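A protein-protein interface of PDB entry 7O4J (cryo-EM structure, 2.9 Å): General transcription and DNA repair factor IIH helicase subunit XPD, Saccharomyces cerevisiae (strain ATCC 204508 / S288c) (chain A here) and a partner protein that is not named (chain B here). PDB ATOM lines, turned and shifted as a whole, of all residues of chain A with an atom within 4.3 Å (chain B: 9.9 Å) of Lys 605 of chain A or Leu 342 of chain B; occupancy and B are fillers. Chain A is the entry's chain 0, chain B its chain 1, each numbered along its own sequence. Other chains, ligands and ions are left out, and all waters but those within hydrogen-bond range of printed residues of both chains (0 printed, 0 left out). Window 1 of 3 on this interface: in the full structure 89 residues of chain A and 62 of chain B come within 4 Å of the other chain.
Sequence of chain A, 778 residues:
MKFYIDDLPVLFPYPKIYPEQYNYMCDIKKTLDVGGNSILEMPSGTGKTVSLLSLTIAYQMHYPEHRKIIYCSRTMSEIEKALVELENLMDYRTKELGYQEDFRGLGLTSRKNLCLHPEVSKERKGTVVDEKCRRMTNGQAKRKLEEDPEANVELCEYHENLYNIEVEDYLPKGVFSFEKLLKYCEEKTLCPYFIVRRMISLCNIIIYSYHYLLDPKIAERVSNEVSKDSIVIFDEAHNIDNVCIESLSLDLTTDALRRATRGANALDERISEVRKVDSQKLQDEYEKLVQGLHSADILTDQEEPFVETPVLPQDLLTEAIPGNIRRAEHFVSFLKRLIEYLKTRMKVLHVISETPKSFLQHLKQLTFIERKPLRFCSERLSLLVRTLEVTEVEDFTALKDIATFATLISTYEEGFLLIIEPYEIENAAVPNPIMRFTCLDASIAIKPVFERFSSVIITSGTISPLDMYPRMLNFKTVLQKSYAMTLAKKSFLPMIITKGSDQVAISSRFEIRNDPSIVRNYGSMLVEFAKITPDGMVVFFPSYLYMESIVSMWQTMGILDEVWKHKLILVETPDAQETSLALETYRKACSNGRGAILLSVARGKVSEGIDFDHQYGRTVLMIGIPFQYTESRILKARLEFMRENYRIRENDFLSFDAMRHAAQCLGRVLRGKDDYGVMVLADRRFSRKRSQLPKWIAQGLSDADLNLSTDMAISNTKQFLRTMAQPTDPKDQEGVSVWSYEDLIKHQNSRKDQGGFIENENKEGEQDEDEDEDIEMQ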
ATOM      1  N   GLU A 572     -28.722  15.390  -3.090  1.00  0.00           N
ATOM      2  CA  GLU A 572     -27.375  15.203  -3.611  1.00  0.00           C
ATOM      3  C   GLU A 572     -27.464  14.599  -5.007  1.00  0.00           C
ATOM      4  O   GLU A 572     -28.202  13.633  -5.226  1.00  0.00           O
ATOM      5  CB  GLU A 572     -26.568  14.303  -2.678  1.00  0.00           C
ATOM      6  CG  GLU A 572     -25.114  14.110  -3.083  1.00  0.00           C
ATOM      7  CD  GLU A 572     -24.498  12.873  -2.459  1.00  0.00           C
ATOM      8  OE1 GLU A 572     -24.789  11.757  -2.938  1.00  0.00           O
ATOM      9  OE2 GLU A 572     -23.724  13.016  -1.491  1.00  0.00           O
ATOM     10  N   THR A 573     -26.718  15.165  -5.946  1.00  0.00           N
ATOM     11  CA  THR A 573     -26.710  14.728  -7.331  1.00  0.00           C
ATOM     12  C   THR A 573     -25.307  14.308  -7.753  1.00  0.00           C
ATOM     13  O   THR A 573     -24.316  14.707  -7.135  1.00  0.00           O
ATOM     14  CB  THR A 573     -27.208  15.849  -8.253  1.00  0.00           C
ATOM     15  OG1 THR A 573     -26.353  16.992  -8.129  1.00  0.00           O
ATOM     16  CG2 THR A 573     -28.634  16.240  -7.895  1.00  0.00           C
ATOM     17  N   PRO A 574     -25.186  13.488  -8.803  1.00  0.00           N
ATOM     18  CA  PRO A 574     -23.842  13.062  -9.230  1.00  0.00           C
ATOM     19  C   PRO A 574     -22.920  14.224  -9.556  1.00  0.00           C
ATOM     20  O   PRO A 574     -21.719  14.154  -9.270  1.00  0.00           O
ATOM     21  CB  PRO A 574     -24.125  12.192 -10.465  1.00  0.00           C
ATOM     22  CG  PRO A 574     -25.526  12.519 -10.874  1.00  0.00           C
ATOM     23  CD  PRO A 574     -26.240  12.863  -9.615  1.00  0.00           C
ATOM     24  N   ALA A 576     -20.876  17.426  -9.069  1.00  0.00           N
ATOM     25  CA  ALA A 576     -20.327  18.022  -7.857  1.00  0.00           C
ATOM     26  C   ALA A 576     -20.768  19.470  -7.689  1.00  0.00           C
ATOM     27  O   ALA A 576     -21.148  19.882  -6.587  1.00  0.00           O
ATOM     28  CB  ALA A 576     -18.801  17.931  -7.875  1.00  0.00           C
ATOM     29  N   THR A 579     -24.401  19.752  -6.541  1.00  0.00           N
ATOM     30  CA  THR A 579     -24.501  19.430  -5.122  1.00  0.00           C
ATOM     31  C   THR A 579     -23.987  20.572  -4.258  1.00  0.00           C
ATOM     32  O   THR A 579     -24.560  20.854  -3.199  1.00  0.00           O
ATOM     33  CB  THR A 579     -23.729  18.148  -4.811  1.00  0.00           C
ATOM     34  OG1 THR A 579     -24.049  17.144  -5.782  1.00  0.00           O
ATOM     35  CG2 THR A 579     -24.078  17.634  -3.424  1.00  0.00           C
ATOM     36  N   SER A 580     -22.910  21.235  -4.685  1.00  0.00           N
ATOM     37  CA  SER A 580     -22.418  22.390  -3.945  1.00  0.00           C
ATOM     38  C   SER A 580     -23.464  23.495  -3.899  1.00  0.00           C
ATOM     39  O   SER A 580     -23.654  24.135  -2.858  1.00  0.00           O
ATOM     40  CB  SER A 580     -21.123  22.902  -4.574  1.00  0.00           C
ATOM     41  OG  SER A 580     -20.182  21.853  -4.727  1.00  0.00           O
ATOM     42  N   LEU A 583     -25.952  22.515  -1.353  1.00  0.00           N
ATOM     43  CA  LEU A 583     -25.474  22.800  -0.005  1.00  0.00           C
ATOM     44  C   LEU A 583     -25.641  24.278   0.330  1.00  0.00           C
ATOM     45  O   LEU A 583     -26.084  24.631   1.428  1.00  0.00           O
ATOM     46  CB  LEU A 583     -24.010  22.382   0.129  1.00  0.00           C
ATOM     47  CG  LEU A 583     -23.712  20.890   0.296  1.00  0.00           C
ATOM     48  CD1 LEU A 583     -22.234  20.683   0.585  1.00  0.00           C
ATOM     49  CD2 LEU A 583     -24.560  20.266   1.395  1.00  0.00           C
ATOM     50  N   GLY A 604     -21.061   9.223   0.109  1.00  0.00           N
ATOM     51  CA  GLY A 604     -20.965  10.161  -0.978  1.00  0.00           C
ATOM     52  C   GLY A 604     -20.023  11.310  -0.691  1.00  0.00           C
ATOM     53  O   GLY A 604     -19.170  11.251   0.206  1.00  0.00           O
ATOM     54  N   LYS A 605     -20.177  12.382  -1.471  1.00  0.00           N
ATOM     55  CA  LYS A 605     -19.304  13.544  -1.345  1.00  0.00           C
ATOM     56  C   LYS A 605     -19.646  14.373  -0.113  1.00  0.00           C
ATOM     57  O   LYS A 605     -18.764  15.007   0.477  1.00  0.00           O
ATOM     58  CB  LYS A 605     -19.400  14.418  -2.597  1.00  0.00           C
ATOM     59  CG  LYS A 605     -19.331  13.662  -3.916  1.00  0.00           C
ATOM     60  CD  LYS A 605     -19.713  14.557  -5.086  1.00  0.00           C
ATOM     61  CE  LYS A 605     -21.221  14.734  -5.195  1.00  0.00           C
ATOM     62  NZ  LYS A 605     -21.903  13.493  -5.649  1.00  0.00           N
ATOM     63  N   VAL A 606     -20.920  14.399   0.274  1.00  0.00           N
ATOM     64  CA  VAL A 606     -21.338  15.229   1.399  1.00  0.00           C
ATOM     65  C   VAL A 606     -20.768  14.688   2.704  1.00  0.00           C
ATOM     66  O   VAL A 606     -20.387  15.454   3.597  1.00  0.00           O
ATOM     67  CB  VAL A 606     -22.874  15.318   1.445  1.00  0.00           C
ATOM     68  CG1 VAL A 606     -23.325  16.058   2.686  1.00  0.00           C
ATOM     69  CG2 VAL A 606     -23.400  16.000   0.194  1.00  0.00           C
ATOM     70  N   SER A 607     -20.702  13.363   2.836  1.00  0.00           N
ATOM     71  CA  SER A 607     -20.315  12.745   4.098  1.00  0.00           C
ATOM     72  C   SER A 607     -18.816  12.792   4.361  1.00  0.00           C
ATOM     73  O   SER A 607     -18.396  12.455   5.473  1.00  0.00           O
ATOM     74  CB  SER A 607     -20.786  11.291   4.125  1.00  0.00           C
ATOM     75  OG  SER A 607     -20.005  10.488   3.257  1.00  0.00           O
ATOM     76  N   GLU A 608     -18.002  13.194   3.387  1.00  0.00           N
ATOM     77  CA  GLU A 608     -16.546  13.119   3.506  1.00  0.00           C
ATOM     78  C   GLU A 608     -15.914  14.483   3.758  1.00  0.00           C
ATOM     79  O   GLU A 608     -14.834  14.776   3.233  1.00  0.00           O
ATOM     80  CB  GLU A 608     -15.944  12.470   2.263  1.00  0.00           C
ATOM     81  CG  GLU A 608     -16.143  13.249   0.981  1.00  0.00           C
ATOM     82  CD  GLU A 608     -15.800  12.437  -0.252  1.00  0.00           C
ATOM     83  OE1 GLU A 608     -16.004  12.943  -1.376  1.00  0.00           O
ATOM     84  OE2 GLU A 608     -15.331  11.289  -0.098  1.00  0.00           O
ATOM     85  N   ILE A 610     -18.115  17.656   4.763  1.00  0.00           N
ATOM     86  CA  ILE A 610     -19.088  18.702   5.056  1.00  0.00           C
ATOM     87  C   ILE A 610     -19.713  18.447   6.421  1.00  0.00           C
ATOM     88  O   ILE A 610     -20.173  17.336   6.719  1.00  0.00           O
ATOM     89  CB  ILE A 610     -20.159  18.765   3.954  1.00  0.00           C
ATOM     90  CG1 ILE A 610     -19.508  19.018   2.590  1.00  0.00           C
ATOM     91  CG2 ILE A 610     -21.185  19.846   4.269  1.00  0.00           C
ATOM     92  CD1 ILE A 610     -18.704  20.303   2.507  1.00  0.00           C
ATOM     93  N   PRO B 335     -19.688  30.921  -8.429  1.00  0.00           N
ATOM     94  CA  PRO B 335     -18.595  30.322  -7.654  1.00  0.00           C
ATOM     95  C   PRO B 335     -19.015  30.074  -6.213  1.00  0.00           C
ATOM     96  O   PRO B 335     -19.713  30.884  -5.600  1.00  0.00           O
ATOM     97  CB  PRO B 335     -17.472  31.364  -7.750  1.00  0.00           C
ATOM     98  CG  PRO B 335     -18.143  32.631  -8.170  1.00  0.00           C
ATOM     99  CD  PRO B 335     -19.301  32.214  -9.015  1.00  0.00           C
ATOM    100  N   VAL B 336     -18.578  28.939  -5.677  1.00  0.00           N
ATOM    101  CA  VAL B 336     -18.945  28.503  -4.335  1.00  0.00           C
ATOM    102  C   VAL B 336     -17.745  28.676  -3.418  1.00  0.00           C
ATOM    103  O   VAL B 336     -16.593  28.540  -3.848  1.00  0.00           O
ATOM    104  CB  VAL B 336     -19.429  27.039  -4.343  1.00  0.00           C
ATOM    105  CG1 VAL B 336     -19.631  26.532  -2.922  1.00  0.00           C
ATOM    106  CG2 VAL B 336     -20.711  26.909  -5.149  1.00  0.00           C
ATOM    107  N   LYS B 337     -18.014  28.979  -2.150  1.00  0.00           N
ATOM    108  CA  LYS B 337     -16.941  29.116  -1.177  1.00  0.00           C
ATOM    109  C   LYS B 337     -16.183  27.801  -1.041  1.00  0.00           C
ATOM    110  O   LYS B 337     -16.762  26.713  -1.090  1.00  0.00           O
ATOM    111  CB  LYS B 337     -17.502  29.542   0.180  1.00  0.00           C
ATOM    112  CG  LYS B 337     -18.070  30.952   0.200  1.00  0.00           C
ATOM    113  CD  LYS B 337     -18.509  31.366   1.599  1.00  0.00           C
ATOM    114  CE  LYS B 337     -19.729  30.585   2.070  1.00  0.00           C
ATOM    115  NZ  LYS B 337     -20.921  30.826   1.212  1.00  0.00           N
ATOM    116  N   LYS B 338     -14.865  27.910  -0.864  1.00  0.00           N
ATOM    117  CA  LYS B 338     -14.023  26.725  -0.775  1.00  0.00           C
ATOM    118  C   LYS B 338     -14.360  25.865   0.437  1.00  0.00           C
ATOM    119  O   LYS B 338     -13.991  24.687   0.465  1.00  0.00           O
ATOM    120  CB  LYS B 338     -12.551  27.133  -0.723  1.00  0.00           C
ATOM    121  CG  LYS B 338     -12.030  27.753  -2.008  1.00  0.00           C
ATOM    122  CD  LYS B 338     -11.739  26.698  -3.061  1.00  0.00           C
ATOM    123  CE  LYS B 338     -11.219  27.323  -4.344  1.00  0.00           C
ATOM    124  NZ  LYS B 338     -11.422  26.435  -5.520  1.00  0.00           N
ATOM    125  N   ILE B 339     -15.049  26.423   1.434  1.00  0.00           N
ATOM    126  CA  ILE B 339     -15.372  25.659   2.637  1.00  0.00           C
ATOM    127  C   ILE B 339     -16.259  24.471   2.288  1.00  0.00           C
ATOM    128  O   ILE B 339     -16.038  23.349   2.761  1.00  0.00           O
ATOM    129  CB  ILE B 339     -16.039  26.567   3.685  1.00  0.00           C
ATOM    130  CG1 ILE B 339     -15.095  27.699   4.105  1.00  0.00           C
ATOM    131  CG2 ILE B 339     -16.467  25.754   4.898  1.00  0.00           C
ATOM    132  CD1 ILE B 339     -13.787  27.232   4.712  1.00  0.00           C
ATOM    133  N   ILE B 340     -17.275  24.697   1.461  1.00  0.00           N
ATOM    134  CA  ILE B 340     -18.216  23.655   1.075  1.00  0.00           C
ATOM    135  C   ILE B 340     -18.168  23.392  -0.430  1.00  0.00           C
ATOM    136  O   ILE B 340     -19.165  22.978  -1.018  1.00  0.00           O
ATOM    137  CB  ILE B 340     -19.642  23.996   1.537  1.00  0.00           C
ATOM    138  CG1 ILE B 340     -20.142  25.280   0.871  1.00  0.00           C
ATOM    139  CG2 ILE B 340     -19.688  24.135   3.050  1.00  0.00           C
ATOM    140  CD1 ILE B 340     -21.628  25.504   1.040  1.00  0.00           C
ATOM    141  N   ASP B 341     -17.021  23.630  -1.063  1.00  0.00           N
ATOM    142  CA  ASP B 341     -16.867  23.385  -2.492  1.00  0.00           C
ATOM    143  C   ASP B 341     -16.565  21.908  -2.711  1.00  0.00           C
ATOM    144  O   ASP B 341     -15.429  21.465  -2.523  1.00  0.00           O
ATOM    145  CB  ASP B 341     -15.757  24.261  -3.067  1.00  0.00           C
ATOM    146  CG  ASP B 341     -15.491  23.977  -4.531  1.00  0.00           C
ATOM    147  OD1 ASP B 341     -16.464  23.755  -5.282  1.00  0.00           O
ATOM    148  OD2 ASP B 341     -14.308  23.974  -4.931  1.00  0.00           O
ATOM    149  N   LEU B 342     -17.581  21.145  -3.114  1.00  0.00           N
ATOM    150  CA  LEU B 342     -17.406  19.723  -3.371  1.00  0.00           C
ATOM    151  C   LEU B 342     -16.714  19.443  -4.697  1.00  0.00           C
ATOM    152  O   LEU B 342     -16.191  18.339  -4.881  1.00  0.00           O
ATOM    153  CB  LEU B 342     -18.762  19.015  -3.347  1.00  0.00           C
ATOM    154  CG  LEU B 342     -19.524  19.099  -2.023  1.00  0.00           C
ATOM    155  CD1 LEU B 342     -20.942  18.582  -2.189  1.00  0.00           C
ATOM    156  CD2 LEU B 342     -18.793  18.329  -0.935  1.00  0.00           C
ATOM    157  N   ASP B 343     -16.695  20.407  -5.619  1.00  0.00           N
ATOM    158  CA  ASP B 343     -16.010  20.201  -6.889  1.00  0.00           C
ATOM    159  C   ASP B 343     -14.502  20.115  -6.714  1.00  0.00           C
ATOM    160  O   ASP B 343     -13.848  19.322  -7.400  1.00  0.00           O
ATOM    161  CB  ASP B 343     -16.355  21.327  -7.865  1.00  0.00           C
ATOM    162  CG  ASP B 343     -16.149  20.927  -9.313  1.00  0.00           C
ATOM    163  OD1 ASP B 343     -15.745  19.772  -9.563  1.00  0.00           O
ATOM    164  OD2 ASP B 343     -16.387  21.770 -10.204  1.00  0.00           O
ATOM    165  N   GLY B 344     -13.932  20.912  -5.809  1.00  0.00           N
ATOM    166  CA  GLY B 344     -12.500  20.862  -5.585  1.00  0.00           C
ATOM    167  C   GLY B 344     -12.031  19.587  -4.921  1.00  0.00           C
ATOM    168  O   GLY B 344     -10.865  19.211  -5.079  1.00  0.00           O
ATOM    169  N   ASN B 345     -12.913  18.910  -4.183  1.00  0.00           N
ATOM    170  CA  ASN B 345     -12.535  17.648  -3.558  1.00  0.00           C
ATOM    171  C   ASN B 345     -12.316  16.561  -4.602  1.00  0.00           C
ATOM    172  O   ASN B 345     -11.394  15.747  -4.475  1.00  0.00           O
ATOM    173  CB  ASN B 345     -13.605  17.224  -2.553  1.00  0.00           C
ATOM    174  CG  ASN B 345     -13.852  18.272  -1.489  1.00  0.00           C
ATOM    175  OD1 ASN B 345     -13.010  19.135  -1.245  1.00  0.00           O
ATOM    176  ND2 ASN B 345     -15.012  18.204  -0.848  1.00  0.00           N
ATOM    177  N   ILE B 346     -13.154  16.529  -5.641  1.00  0.00           N
ATOM    178  CA  ILE B 346     -12.983  15.539  -6.698  1.00  0.00           C
ATOM    179  C   ILE B 346     -11.869  15.924  -7.663  1.00  0.00           C
ATOM    180  O   ILE B 346     -11.330  15.050  -8.354  1.00  0.00           O
ATOM    181  CB  ILE B 346     -14.306  15.322  -7.455  1.00  0.00           C
ATOM    182  CG1 ILE B 346     -14.755  16.602  -8.167  1.00  0.00           C
ATOM    183  CG2 ILE B 346     -15.390  14.845  -6.500  1.00  0.00           C
ATOM    184  CD1 ILE B 346     -15.654  16.349  -9.356  1.00  0.00           C
ATOM    185  N   GLN B 347     -11.509  17.206  -7.730  1.00  0.00           N
ATOM    186  CA  GLN B 347     -10.391  17.673  -8.538  1.00  0.00           C
ATOM    187  C   GLN B 347      -9.118  17.838  -7.717  1.00  0.00           C
ATOM    188  O   GLN B 347      -8.118  18.349  -8.232  1.00  0.00           O
ATOM    189  CB  GLN B 347     -10.748  18.993  -9.223  1.00  0.00           C
ATOM    190  CG  GLN B 347     -12.007  18.938 -10.071  1.00  0.00           C
ATOM    191  CD  GLN B 347     -11.889  17.966 -11.228  1.00  0.00           C
ATOM    192  OE1 GLN B 347     -10.800  17.740 -11.755  1.00  0.00           O
ATOM    193  NE2 GLN B 347     -13.014  17.386 -11.630  1.00  0.00           N
ATOM    194  N   ASP B 348      -9.133  17.418  -6.450  1.00  0.00           N
ATOM    195  CA  ASP B 348      -7.947  17.539  -5.609  1.00  0.00           C
ATOM    196  C   ASP B 348      -6.760  16.822  -6.241  1.00  0.00           C
ATOM    197  O   ASP B 348      -5.653  17.368  -6.320  1.00  0.00           O
ATOM    198  CB  ASP B 348      -8.237  16.980  -4.217  1.00  0.00           C
ATOM    199  CG  ASP B 348      -7.563  17.772  -3.114  1.00  0.00           C
ATOM    200  OD1 ASP B 348      -6.568  18.471  -3.402  1.00  0.00           O
ATOM    201  OD2 ASP B 348      -8.027  17.694  -1.957  1.00  0.00           O
ATOM    202  N   ASP B 349      -6.974  15.590  -6.690  1.00  0.00           N
ATOM    203  CA  ASP B 349      -5.963  14.837  -7.422  1.00  0.00           C
ATOM    204  C   ASP B 349      -6.527  14.465  -8.786  1.00  0.00           C
ATOM    205  O   ASP B 349      -7.341  13.532  -8.877  1.00  0.00           O
ATOM    206  CB  ASP B 349      -5.556  13.584  -6.644  1.00  0.00           C
ATOM    207  CG  ASP B 349      -4.536  12.742  -7.385  1.00  0.00           C
ATOM    208  OD1 ASP B 349      -3.986  13.223  -8.398  1.00  0.00           O
ATOM    209  OD2 ASP B 349      -4.285  11.597  -6.955  1.00  0.00           O
ATOM    210  N   MET B 361     -23.780   2.731  -6.699  1.00  0.00           N
ATOM    211  CA  MET B 361     -23.233   4.060  -6.457  1.00  0.00           C
ATOM    212  C   MET B 361     -23.279   4.934  -7.705  1.00  0.00           C
ATOM    213  O   MET B 361     -22.534   5.916  -7.804  1.00  0.00           O
ATOM    214  CB  MET B 361     -21.796   3.947  -5.944  1.00  0.00           C
ATOM    215  CG  MET B 361     -21.665   3.409  -4.523  1.00  0.00           C
ATOM    216  SD  MET B 361     -22.726   4.230  -3.314  1.00  0.00           S
ATOM    217  CE  MET B 361     -22.294   5.946  -3.594  1.00  0.00           C
ATOM    218  N   GLN B 362     -24.139   4.600  -8.657  1.00  0.00           N
ATOM    219  CA  GLN B 362     -24.274   5.332  -9.904  1.00  0.00           C
ATOM    220  C   GLN B 362     -25.752   5.546 -10.187  1.00  0.00           C
ATOM    221  O   GLN B 362     -26.599   4.803  -9.679  1.00  0.00           O
ATOM    222  CB  GLN B 362     -23.625   4.580 -11.073  1.00  0.00           C
ATOM    223  CG  GLN B 362     -22.108   4.607 -11.064  1.00  0.00           C
ATOM    224  CD  GLN B 362     -21.511   4.069 -12.347  1.00  0.00           C
ATOM    225  OE1 GLN B 362     -22.165   3.341 -13.094  1.00  0.00           O
ATOM    226  NE2 GLN B 362     -20.259   4.427 -12.612  1.00  0.00           N
ATOM    227  N   PRO B 363     -26.093   6.553 -10.986  1.00  0.00           N
ATOM    228  CA  PRO B 363     -27.498   6.744 -11.359  1.00  0.00           C
ATOM    229  C   PRO B 363     -28.045   5.536 -12.101  1.00  0.00           C
ATOM    230  O   PRO B 363     -27.345   4.882 -12.877  1.00  0.00           O
ATOM    231  CB  PRO B 363     -27.467   7.984 -12.260  1.00  0.00           C
ATOM    232  CG  PRO B 363     -26.193   8.676 -11.926  1.00  0.00           C
ATOM    233  CD  PRO B 363     -25.227   7.599 -11.558  1.00  0.00           C
ATOM    234  N   LYS B 379     -33.261  16.673  -9.781  1.00  0.00           N
ATOM    235  CA  LYS B 379     -32.813  18.011 -10.147  1.00  0.00           C
ATOM    236  C   LYS B 379     -33.971  18.999 -10.164  1.00  0.00           C
ATOM    237  O   LYS B 379     -33.796  20.167  -9.801  1.00  0.00           O
ATOM    238  CB  LYS B 379     -32.127  17.978 -11.513  1.00  0.00           C
ATOM    239  CG  LYS B 379     -30.805  17.230 -11.523  1.00  0.00           C
ATOM    240  CD  LYS B 379     -30.129  17.307 -12.881  1.00  0.00           C
ATOM    241  CE  LYS B 379     -28.943  16.358 -12.965  1.00  0.00           C
ATOM    242  NZ  LYS B 379     -27.859  16.722 -12.011  1.00  0.00           N
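OG of Ser 580 of chain A is in hydrogen-bond range of N of Leu 342 of chain B (3.1 Å).
The backbone carbonyl oxygen (O) of Thr 573 of chain A is in hydrogen-bond range of the side-chain hydroxyl (OG1) of Thr 579 of chain A (2.8 Å).
The backbone carbonyl oxygen (O) of Thr 573 of chain A sits at hydrogen-bond distance from the side-chain amino group (NZ) of Lys 605 of chain A (3.1 Å).
The backbone carbonyl oxygen of Ala 576 of chain A is in hydrogen-bond range of the side-chain hydroxyl of Ser 580 of chain A (2.9 Å).
The side-chain carboxylate of Asp 341 of chain B lies close to the backbone NH of Asp 343 of chain B, at 3.4 Å.
CB of Thr 573 of chain A touches NZ of Lys 379 of chain B, 3.9 Å away.
CB of Ala 576 of chain A touches O of Leu 342 of chain B, at 3.99 Å.
Asp 343 of chain B touches Ala 576 of chain A.
Ala 576 of chain A touches Ile 346 of chain B.
CD1 of Leu 342 of chain B touches CG2 of Thr 579 of chain A, at 3.5 Å.
Ser 580 of chain A touches Asp 343 of chain B.
CD1 of Leu 583 of chain A touches CD1 of Leu 342 of chain B, 3.7 Å away.
Leu 342 of chain B touches Lys 605 of chain A.
CA of Ile 340 of chain B touches CD1 of Ile 610 of chain A, 3.7 Å away.
Ile 610 of chain A touches Leu 342 of chain B.
Of the printed residues of chain B, Ala 576 of chain A touches Leu 342 (3.99 Å), Asp 343 (3.7 Å) and Ile 346 (3.8 Å).
Thr 579 of chain A touches just one residue of chain B: Leu 342 (3.5 Å).
Of the printed residues of chain B, Leu 583 of chain A touches Leu 342 (3.7 Å).
No residue of chain B comes within 4 Å of Gly 604 of chain A.
Lys 605 of chain A touches one residue of chain B.
No residue of chain B comes within 4 Å of Val 606 of chain A.
Glu 608 of chain A touches none of the printed residues of chain B.
Of the printed residues of chain A, Ile 340 of chain B touches Ile 610.
Of the printed residues of chain A, Leu 342 of chain B touches Ala 576 (3.99 Å), Thr 579 (3.5 Å), Ser 580 (3.1 Å), Leu 583 (3.7 Å), Lys 605 (3.6 Å) and Ile 610 (3.7 Å).
The nearest residue of chain B that does not touch Lys 605 of chain A is Ile 346 of chain B (4.6 Å).
The nearest printed residue of chain B that does not touch Ser 580 of chain A is Ile 340 of chain B (4.01 Å).
Of the 13 printed residues of chain A, 7 touch a printed residue of chain B.
Hydrophobic or aromatic side chains of chain A within 4 Å of the printed part of chain B: Ala 576, Leu 583 and Ile 610.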
